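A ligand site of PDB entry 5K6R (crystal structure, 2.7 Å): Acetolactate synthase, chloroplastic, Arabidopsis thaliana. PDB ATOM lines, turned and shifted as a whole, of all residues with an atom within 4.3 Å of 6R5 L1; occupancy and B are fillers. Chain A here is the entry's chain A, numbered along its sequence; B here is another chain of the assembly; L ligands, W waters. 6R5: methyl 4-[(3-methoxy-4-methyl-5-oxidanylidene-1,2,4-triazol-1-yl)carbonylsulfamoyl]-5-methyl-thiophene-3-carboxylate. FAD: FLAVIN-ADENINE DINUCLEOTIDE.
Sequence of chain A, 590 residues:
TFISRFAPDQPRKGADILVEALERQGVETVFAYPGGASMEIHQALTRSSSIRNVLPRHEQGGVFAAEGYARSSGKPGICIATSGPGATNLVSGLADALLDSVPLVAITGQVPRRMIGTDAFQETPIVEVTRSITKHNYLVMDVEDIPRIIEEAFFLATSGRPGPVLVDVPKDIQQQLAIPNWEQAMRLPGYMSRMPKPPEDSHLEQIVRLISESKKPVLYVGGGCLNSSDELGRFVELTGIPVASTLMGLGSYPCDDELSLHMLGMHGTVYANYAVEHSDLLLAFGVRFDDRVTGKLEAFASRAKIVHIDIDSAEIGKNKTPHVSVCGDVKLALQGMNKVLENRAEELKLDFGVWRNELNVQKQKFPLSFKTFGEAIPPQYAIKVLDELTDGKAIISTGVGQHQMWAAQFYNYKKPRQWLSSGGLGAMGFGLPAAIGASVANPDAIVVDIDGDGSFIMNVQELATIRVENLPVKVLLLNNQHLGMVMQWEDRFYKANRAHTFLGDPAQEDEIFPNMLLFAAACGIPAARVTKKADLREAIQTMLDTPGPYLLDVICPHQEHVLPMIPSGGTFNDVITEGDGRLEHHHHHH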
ATOM      1  N   MET A 266     -15.292 -18.333  -6.841  1.00  0.00           N
ATOM      2  CA  MET A 266     -16.299 -19.208  -7.441  1.00  0.00           C
ATOM      3  C   MET A 266     -15.702 -20.200  -8.445  1.00  0.00           C
ATOM      4  O   MET A 266     -16.036 -21.381  -8.440  1.00  0.00           O
ATOM      5  CB  MET A 266     -17.384 -18.368  -8.121  1.00  0.00           C
ATOM      6  CG  MET A 266     -18.420 -19.179  -8.886  1.00  0.00           C
ATOM      7  SD  MET A 266     -19.844 -18.190  -9.390  1.00  0.00           S
ATOM      8  CE  MET A 266     -20.587 -17.858  -7.797  1.00  0.00           C
ATOM      9  N   ASP A 291     -18.664 -11.263  -3.301  1.00  0.00           N
ATOM     10  CA  ASP A 291     -19.289 -12.568  -3.031  1.00  0.00           C
ATOM     11  C   ASP A 291     -18.825 -13.658  -3.988  1.00  0.00           C
ATOM     12  O   ASP A 291     -18.951 -14.847  -3.665  1.00  0.00           O
ATOM     13  CB  ASP A 291     -20.813 -12.438  -3.086  1.00  0.00           C
ATOM     14  CG  ASP A 291     -21.330 -12.191  -4.496  1.00  0.00           C
ATOM     15  OD1 ASP A 291     -21.302 -11.029  -4.938  1.00  0.00           O
ATOM     16  OD2 ASP A 291     -21.777 -13.160  -5.139  1.00  0.00           O
ATOM     17  N   ARG A 292     -18.298 -13.289  -5.152  1.00  0.00           N
ATOM     18  CA  ARG A 292     -17.690 -14.273  -6.052  1.00  0.00           C
ATOM     19  C   ARG A 292     -16.537 -14.963  -5.346  1.00  0.00           C
ATOM     20  O   ARG A 292     -16.269 -16.153  -5.567  1.00  0.00           O
ATOM     21  CB  ARG A 292     -17.191 -13.628  -7.346  1.00  0.00           C
ATOM     22  CG  ARG A 292     -18.225 -12.897  -8.187  1.00  0.00           C
ATOM     23  CD  ARG A 292     -19.349 -13.797  -8.641  1.00  0.00           C
ATOM     24  NE  ARG A 292     -20.532 -13.645  -7.803  1.00  0.00           N
ATOM     25  CZ  ARG A 292     -21.692 -14.226  -8.043  1.00  0.00           C
ATOM     26  NH1 ARG A 292     -21.821 -15.019  -9.106  1.00  0.00           N
ATOM     27  NH2 ARG A 292     -22.724 -14.029  -7.232  1.00  0.00           N
ATOM     28  N   TRP A 489     -25.284 -22.988 -16.336  1.00  0.00           N
ATOM     29  CA  TRP A 489     -26.211 -22.857 -15.218  1.00  0.00           C
ATOM     30  C   TRP A 489     -27.524 -23.591 -15.487  1.00  0.00           C
ATOM     31  O   TRP A 489     -28.167 -24.092 -14.566  1.00  0.00           O
ATOM     32  CB  TRP A 489     -26.465 -21.388 -14.902  1.00  0.00           C
ATOM     33  CG  TRP A 489     -25.418 -20.782 -14.034  1.00  0.00           C
ATOM     34  CD1 TRP A 489     -24.098 -20.617 -14.327  1.00  0.00           C
ATOM     35  CD2 TRP A 489     -25.604 -20.258 -12.711  1.00  0.00           C
ATOM     36  NE1 TRP A 489     -23.444 -20.032 -13.270  1.00  0.00           N
ATOM     37  CE2 TRP A 489     -24.339 -19.793 -12.265  1.00  0.00           C
ATOM     38  CE3 TRP A 489     -26.703 -20.136 -11.860  1.00  0.00           C
ATOM     39  CZ2 TRP A 489     -24.162 -19.222 -11.014  1.00  0.00           C
ATOM     40  CZ3 TRP A 489     -26.519 -19.561 -10.615  1.00  0.00           C
ATOM     41  CH2 TRP A 489     -25.256 -19.111 -10.198  1.00  0.00           C
ATOM     42  N   SER A 568     -23.193 -20.163  -5.919  1.00  0.00           N
ATOM     43  CA  SER A 568     -23.369 -18.834  -5.344  1.00  0.00           C
ATOM     44  C   SER A 568     -23.917 -18.894  -3.919  1.00  0.00           C
ATOM     45  O   SER A 568     -24.970 -19.485  -3.677  1.00  0.00           O
ATOM     46  CB  SER A 568     -24.298 -17.994  -6.225  1.00  0.00           C
ATOM     47  OG  SER A 568     -24.413 -16.671  -5.733  1.00  0.00           O
ATOM     48  N   GLY B  36     -27.963 -13.990 -15.873  1.00  0.00           N
ATOM     49  CA  GLY B  36     -28.092 -14.619 -14.578  1.00  0.00           C
ATOM     50  C   GLY B  36     -29.292 -14.182 -13.749  1.00  0.00           C
ATOM     51  O   GLY B  36     -30.019 -15.022 -13.200  1.00  0.00           O
ATOM     52  N   ALA B  37     -29.514 -12.876 -13.670  1.00  0.00           N
ATOM     53  CA  ALA B  37     -30.572 -12.339 -12.824  1.00  0.00           C
ATOM     54  C   ALA B  37     -31.963 -12.496 -13.430  1.00  0.00           C
ATOM     55  O   ALA B  37     -32.957 -12.195 -12.778  1.00  0.00           O
ATOM     56  CB  ALA B  37     -30.287 -10.874 -12.518  1.00  0.00           C
ATOM     57  N   MET B  39     -32.715 -15.455 -15.494  1.00  0.00           N
ATOM     58  CA  MET B  39     -32.837 -16.832 -15.969  1.00  0.00           C
ATOM     59  C   MET B  39     -34.200 -17.438 -15.637  1.00  0.00           C
ATOM     60  O   MET B  39     -34.790 -18.129 -16.463  1.00  0.00           O
ATOM     61  CB  MET B  39     -31.728 -17.712 -15.372  1.00  0.00           C
ATOM     62  CG  MET B  39     -30.355 -17.476 -15.965  1.00  0.00           C
ATOM     63  SD  MET B  39     -29.179 -18.758 -15.493  1.00  0.00           S
ATOM     64  CE  MET B  39     -29.909 -20.182 -16.299  1.00  0.00           C
ATOM     65  N   VAL B 111     -30.412  -8.335  -8.830  1.00  0.00           N
ATOM     66  CA  VAL B 111     -29.831  -9.157  -7.782  1.00  0.00           C
ATOM     67  C   VAL B 111     -30.838  -9.365  -6.655  1.00  0.00           C
ATOM     68  O   VAL B 111     -31.811  -8.594  -6.543  1.00  0.00           O
ATOM     69  CB  VAL B 111     -28.550  -8.508  -7.214  1.00  0.00           C
ATOM     70  CG1 VAL B 111     -27.535  -8.289  -8.323  1.00  0.00           C
ATOM     71  CG2 VAL B 111     -28.866  -7.198  -6.514  1.00  0.00           C
ATOM     72  N   PRO B 112     -30.647 -10.398  -5.828  1.00  0.00           N
ATOM     73  CA  PRO B 112     -31.524 -10.600  -4.659  1.00  0.00           C
ATOM     74  C   PRO B 112     -31.661  -9.336  -3.804  1.00  0.00           C
ATOM     75  O   PRO B 112     -30.740  -8.524  -3.775  1.00  0.00           O
ATOM     76  CB  PRO B 112     -30.816 -11.716  -3.885  1.00  0.00           C
ATOM     77  CG  PRO B 112     -30.115 -12.505  -4.937  1.00  0.00           C
ATOM     78  CD  PRO B 112     -29.684 -11.511  -5.986  1.00  0.00           C
ATOM     79  N   ARG B 114     -31.539  -8.694  -0.631  1.00  0.00           N
ATOM     80  CA  ARG B 114     -30.563  -8.495   0.433  1.00  0.00           C
ATOM     81  C   ARG B 114     -29.221  -7.992  -0.109  1.00  0.00           C
ATOM     82  O   ARG B 114     -28.429  -7.418   0.632  1.00  0.00           O
ATOM     83  CB  ARG B 114     -30.356  -9.786   1.217  1.00  0.00           C
ATOM     84  CG  ARG B 114     -29.512 -10.819   0.488  1.00  0.00           C
ATOM     85  CD  ARG B 114     -29.383 -12.118   1.273  1.00  0.00           C
ATOM     86  NE  ARG B 114     -28.345 -12.977   0.706  1.00  0.00           N
ATOM     87  CZ  ARG B 114     -28.523 -13.763  -0.344  1.00  0.00           C
ATOM     88  NH1 ARG B 114     -29.701 -13.807  -0.958  1.00  0.00           N
ATOM     89  NH2 ARG B 114     -27.523 -14.505  -0.796  1.00  0.00           N
ATOM     90  N   MET B 115     -28.979  -8.222  -1.395  1.00  0.00           N
ATOM     91  CA  MET B 115     -27.705  -7.868  -2.016  1.00  0.00           C
ATOM     92  C   MET B 115     -27.712  -6.442  -2.553  1.00  0.00           C
ATOM     93  O   MET B 115     -26.653  -5.913  -2.913  1.00  0.00           O
ATOM     94  CB  MET B 115     -27.374  -8.833  -3.156  1.00  0.00           C
ATOM     95  CG  MET B 115     -27.195 -10.288  -2.718  1.00  0.00           C
ATOM     96  SD  MET B 115     -25.832 -10.503  -1.551  1.00  0.00           S
ATOM     97  CE  MET B 115     -24.453  -9.883  -2.519  1.00  0.00           C
ATOM     98  N   ALA B 120     -22.995  -5.429  -5.552  1.00  0.00           N
ATOM     99  CA  ALA B 120     -22.929  -6.867  -5.804  1.00  0.00           C
ATOM    100  C   ALA B 120     -22.613  -7.179  -7.257  1.00  0.00           C
ATOM    101  O   ALA B 120     -22.509  -6.283  -8.103  1.00  0.00           O
ATOM    102  CB  ALA B 120     -24.244  -7.523  -5.394  1.00  0.00           C
ATOM    103  N   PHE B 121     -22.446  -8.471  -7.547  1.00  0.00           N
ATOM    104  CA  PHE B 121     -22.130  -8.937  -8.895  1.00  0.00           C
ATOM    105  C   PHE B 121     -23.228  -8.570  -9.880  1.00  0.00           C
ATOM    106  O   PHE B 121     -24.390  -8.951  -9.702  1.00  0.00           O
ATOM    107  CB  PHE B 121     -21.891 -10.444  -8.895  1.00  0.00           C
ATOM    108  CG  PHE B 121     -21.625 -11.021 -10.256  1.00  0.00           C
ATOM    109  CD1 PHE B 121     -20.549 -10.592 -11.002  1.00  0.00           C
ATOM    110  CD2 PHE B 121     -22.458 -11.996 -10.779  1.00  0.00           C
ATOM    111  CE1 PHE B 121     -20.305 -11.114 -12.269  1.00  0.00           C
ATOM    112  CE2 PHE B 121     -22.221 -12.522 -12.040  1.00  0.00           C
ATOM    113  CZ  PHE B 121     -21.144 -12.085 -12.779  1.00  0.00           C
ATOM    114  N   GLN B 122     -22.850  -7.831 -10.918  1.00  0.00           N
ATOM    115  CA  GLN B 122     -23.760  -7.376 -11.957  1.00  0.00           C
ATOM    116  C   GLN B 122     -24.936  -6.585 -11.382  1.00  0.00           C
ATOM    117  O   GLN B 122     -26.074  -6.736 -11.828  1.00  0.00           O
ATOM    118  CB  GLN B 122     -24.290  -8.559 -12.773  1.00  0.00           C
ATOM    119  CG  GLN B 122     -23.209  -9.318 -13.529  1.00  0.00           C
ATOM    120  CD  GLN B 122     -23.778 -10.215 -14.617  1.00  0.00           C
ATOM    121  OE1 GLN B 122     -24.822 -10.846 -14.439  1.00  0.00           O
ATOM    122  NE2 GLN B 122     -23.087 -10.264 -15.748  1.00  0.00           N
ATOM    123  N   LYS B 171     -34.058 -11.246  -8.103  1.00  0.00           N
ATOM    124  CA  LYS B 171     -34.029 -12.675  -8.428  1.00  0.00           C
ATOM    125  C   LYS B 171     -34.743 -13.546  -7.407  1.00  0.00           C
ATOM    126  O   LYS B 171     -35.382 -14.544  -7.774  1.00  0.00           O
ATOM    127  CB  LYS B 171     -32.577 -13.146  -8.579  1.00  0.00           C
ATOM    128  CG  LYS B 171     -32.433 -14.520  -9.189  1.00  0.00           C
ATOM    129  CD  LYS B 171     -30.982 -14.922  -9.314  1.00  0.00           C
ATOM    130  CE  LYS B 171     -30.831 -16.240 -10.050  1.00  0.00           C
ATOM    131  NZ  LYS B 171     -29.393 -16.554 -10.322  1.00  0.00           N
HETATM  132  C10 6R5 L   1     -26.322 -12.292  -8.098  1.00  0.00           C
HETATM  133  O01 6R5 L   1     -24.641 -15.152  -8.525  1.00  0.00           O
HETATM  134  C02 6R5 L   1     -25.517 -15.473  -9.325  1.00  0.00           C
HETATM  135  N03 6R5 L   1     -26.899 -15.445  -8.913  1.00  0.00           N
HETATM  136  S04 6R5 L   1     -27.258 -14.978  -7.362  1.00  0.00           S
HETATM  137  C05 6R5 L   1     -26.483 -13.407  -7.038  1.00  0.00           C
HETATM  138  C06 6R5 L   1     -25.890 -12.971  -5.775  1.00  0.00           C
HETATM  139  C07 6R5 L   1     -25.832 -13.794  -4.446  1.00  0.00           C
HETATM  140  S08 6R5 L   1     -25.291 -11.471  -5.951  1.00  0.00           S
HETATM  141  C09 6R5 L   1     -25.646 -11.152  -7.525  1.00  0.00           C
HETATM  142  C11 6R5 L   1     -26.819 -12.382  -9.531  1.00  0.00           C
HETATM  143  O12 6R5 L   1     -25.962 -12.099 -10.604  1.00  0.00           O
HETATM  144  C13 6R5 L   1     -26.318 -12.722 -11.799  1.00  0.00           C
HETATM  145  O14 6R5 L   1     -27.968 -12.706  -9.745  1.00  0.00           O
HETATM  146  O15 6R5 L   1     -28.679 -14.913  -7.127  1.00  0.00           O
HETATM  147  O16 6R5 L   1     -26.864 -15.996  -6.413  1.00  0.00           O
HETATM  148  N17 6R5 L   1     -25.109 -15.857 -10.644  1.00  0.00           N
HETATM  149  N18 6R5 L   1     -23.800 -15.904 -11.071  1.00  0.00           N
HETATM  150  C19 6R5 L   1     -23.772 -16.330 -12.438  1.00  0.00           C
HETATM  151  O20 6R5 L   1     -22.624 -16.494 -13.223  1.00  0.00           O
HETATM  152  C21 6R5 L   1     -21.408 -16.238 -12.527  1.00  0.00           C
HETATM  153  N22 6R5 L   1     -25.105 -16.563 -12.835  1.00  0.00           N
HETATM  154  C23 6R5 L   1     -25.524 -17.013 -14.149  1.00  0.00           C
HETATM  155  C24 6R5 L   1     -25.945 -16.278 -11.749  1.00  0.00           C
HETATM  156  O25 6R5 L   1     -27.163 -16.371 -11.728  1.00  0.00           O
HETATM  157  PA  FAD L   2     -11.500  -4.626  -6.995  1.00  0.00           P
HETATM  158  O1A FAD L   2     -10.375  -4.925  -7.997  1.00  0.00           O
HETATM  159  O2A FAD L   2     -12.827  -4.612  -7.719  1.00  0.00           O
HETATM  160  O5B FAD L   2     -11.247  -3.179  -6.313  1.00  0.00           O
HETATM  161  C5B FAD L   2      -9.927  -2.871  -5.798  1.00  0.00           C
HETATM  162  C4B FAD L   2     -10.052  -2.697  -4.286  1.00  0.00           C
HETATM  163  O4B FAD L   2      -8.795  -2.296  -3.720  1.00  0.00           O
HETATM  164  C3B FAD L   2     -11.011  -1.606  -3.950  1.00  0.00           C
HETATM  165  O3B FAD L   2     -11.635  -1.885  -2.693  1.00  0.00           O
HETATM  166  C2B FAD L   2     -10.168  -0.402  -3.849  1.00  0.00           C
HETATM  167  O2B FAD L   2     -10.764   0.532  -2.933  1.00  0.00           O
HETATM  168  C1B FAD L   2      -8.909  -0.913  -3.307  1.00  0.00           C
HETATM  169  N9A FAD L   2      -7.784  -0.197  -3.790  1.00  0.00           N
HETATM  170  C8A FAD L   2      -7.651   0.351  -4.995  1.00  0.00           C
HETATM  171  N7A FAD L   2      -6.445   0.923  -5.081  1.00  0.00           N
HETATM  172  C5A FAD L   2      -5.782   0.735  -3.899  1.00  0.00           C
HETATM  173  C6A FAD L   2      -4.501   1.094  -3.364  1.00  0.00           C
HETATM  174  N6A FAD L   2      -3.598   1.809  -4.135  1.00  0.00           N
HETATM  175  N1A FAD L   2      -4.188   0.722  -2.097  1.00  0.00           N
HETATM  176  C2A FAD L   2      -5.040   0.049  -1.372  1.00  0.00           C
HETATM  177  N3A FAD L   2      -6.255  -0.313  -1.828  1.00  0.00           N
HETATM  178  C4A FAD L   2      -6.641   0.014  -3.077  1.00  0.00           C
HETATM  179  N1  FAD L   2     -13.491 -12.911  -9.135  1.00  0.00           N
HETATM  180  C2  FAD L   2     -12.680 -13.840  -8.404  1.00  0.00           C
HETATM  181  O2  FAD L   2     -11.758 -13.421  -7.723  1.00  0.00           O
HETATM  182  N3  FAD L   2     -12.935 -15.193  -8.464  1.00  0.00           N
HETATM  183  C4  FAD L   2     -13.984 -15.662  -9.247  1.00  0.00           C
HETATM  184  O4  FAD L   2     -14.201 -16.862  -9.297  1.00  0.00           O
HETATM  185  C4X FAD L   2     -14.845 -14.699 -10.033  1.00  0.00           C
HETATM  186  N5  FAD L   2     -15.906 -15.151 -10.820  1.00  0.00           N
HETATM  187  C5X FAD L   2     -16.391 -14.310 -11.773  1.00  0.00           C
HETATM  188  C6  FAD L   2     -17.168 -14.839 -12.825  1.00  0.00           C
HETATM  189  C7  FAD L   2     -17.681 -13.979 -13.816  1.00  0.00           C
HETATM  190  C7M FAD L   2     -18.535 -14.557 -14.960  1.00  0.00           C
HETATM  191  C8  FAD L   2     -17.416 -12.607 -13.749  1.00  0.00           C
HETATM  192  C8M FAD L   2     -17.970 -11.684 -14.835  1.00  0.00           C
HETATM  193  C9  FAD L   2     -16.632 -12.083 -12.709  1.00  0.00           C
HETATM  194  C9A FAD L   2     -16.127 -12.946 -11.712  1.00  0.00           C
HETATM  195  N10 FAD L   2     -15.352 -12.450 -10.666  1.00  0.00           N
HETATM  196  C10 FAD L   2     -14.574 -13.348  -9.956  1.00  0.00           C
HETATM  197  C1' FAD L   2     -15.017 -11.075 -10.613  1.00  0.00           C
HETATM  198  C2' FAD L   2     -15.663 -10.394  -9.376  1.00  0.00           C
HETATM  199  O2' FAD L   2     -17.021 -10.108  -9.673  1.00  0.00           O
HETATM  200  C3' FAD L   2     -14.936  -9.038  -9.011  1.00  0.00           C
HETATM  201  O3' FAD L   2     -14.720  -8.334 -10.150  1.00  0.00           O
HETATM  202  C4' FAD L   2     -13.625  -9.264  -8.306  1.00  0.00           C
HETATM  203  O4' FAD L   2     -13.655 -10.488  -7.565  1.00  0.00           O
HETATM  204  C5' FAD L   2     -13.363  -8.141  -7.346  1.00  0.00           C
HETATM  205  O5' FAD L   2     -12.015  -7.758  -7.448  1.00  0.00           O
HETATM  206  P   FAD L   2     -11.251  -7.250  -6.118  1.00  0.00           P
HETATM  207  O1P FAD L   2     -11.776  -8.029  -4.909  1.00  0.00           O
HETATM  208  O2P FAD L   2      -9.763  -7.497  -6.285  1.00  0.00           O
HETATM  209  O3P FAD L   2     -11.503  -5.721  -5.881  1.00  0.00           O
HETATM  210  O   HOH W   1     -30.250 -17.000  -5.295  1.00  0.00           O
HETATM  211  O   HOH W   2     -23.008 -14.808  -2.898  1.00  0.00           O
HETATM  212  O   HOH W   3     -27.405 -10.714 -14.336  1.00  0.00           O
HETATM  213  O   HOH W   4     -24.994 -15.114  -1.359  1.00  0.00           O
HETATM  214  O   HOH W   5     -27.779 -18.717  -7.378  1.00  0.00           O
HETATM  215  O   HOH W   6     -20.650 -19.390 -12.377  1.00  0.00           O
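Water W6 bridges NE1 of Trp 489 (3.0 Å) and SD of Met 266 (3.3 Å).
Water W3 lies within hydrogen-bond range of the side-chain amide oxygen of Gln 122 of chain B (2.6 Å) and the backbone NH of Ala 37 of chain B (3.1 Å).
NH2 of Arg 292 sits at hydrogen-bond distance from O01 of 6R5 L1.
An oxygen (O4) of FAD L2 sits at hydrogen-bond distance from the backbone NH (N) of Met 266, 3.1 Å away.
The side-chain amino group of Lys 171 of chain B is in hydrogen-bond range of an oxygen (O25) of 6R5 L1, 2.6 Å away.
The side-chain hydroxyl of Ser 568 lies within hydrogen-bond range of an oxygen (O16) of 6R5 L1, 2.6 Å away.
O of Gly 36 of chain B sits close to O25 of 6R5 L1 (3.5 Å).
Asp 291 touches 6R5 L1.
Trp 489 touches 6R5 L1.
N of Ala 37 of chain B touches C13 of 6R5 L1 (3.7 Å).
Val 111 of chain B touches 6R5 L1 (CG1 to C09, 3.5 Å).
Pro 112 of chain B touches 6R5 L1.
CE of Met 115 of chain B touches S08 of 6R5 L1, at 3.9 Å.
O of Phe 121 of chain B touches C09 of 6R5 L1 (3.3 Å).
Gln 122 of chain B touches 6R5 L1 (OE1 to C13, 3.6 Å).
Hydrophobic or aromatic side chains within 4 Å of 6R5 L1: Trp 489, Val 111 of chain B, Pro 112 of chain B, Met 115 of chain B and Phe 121 of chain B.
Of the 16 residues printed, 12 come within 4 Å of 6R5 L1.
O of Arg 292 is in hydrogen-bond range of N of Met 266 (2.7 Å).
The side-chain carboxylate of Asp 291 is in salt-bridge range of the guanidinium group of Arg 292.
The side-chain hydroxyl of Ser 568 is in hydrogen-bond range of the guanidinium group of Arg 292, 3.5 Å away.
NZ of Lys 171 of chain B sits at hydrogen-bond distance from O of Gly 36 of chain B (3.3 Å).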
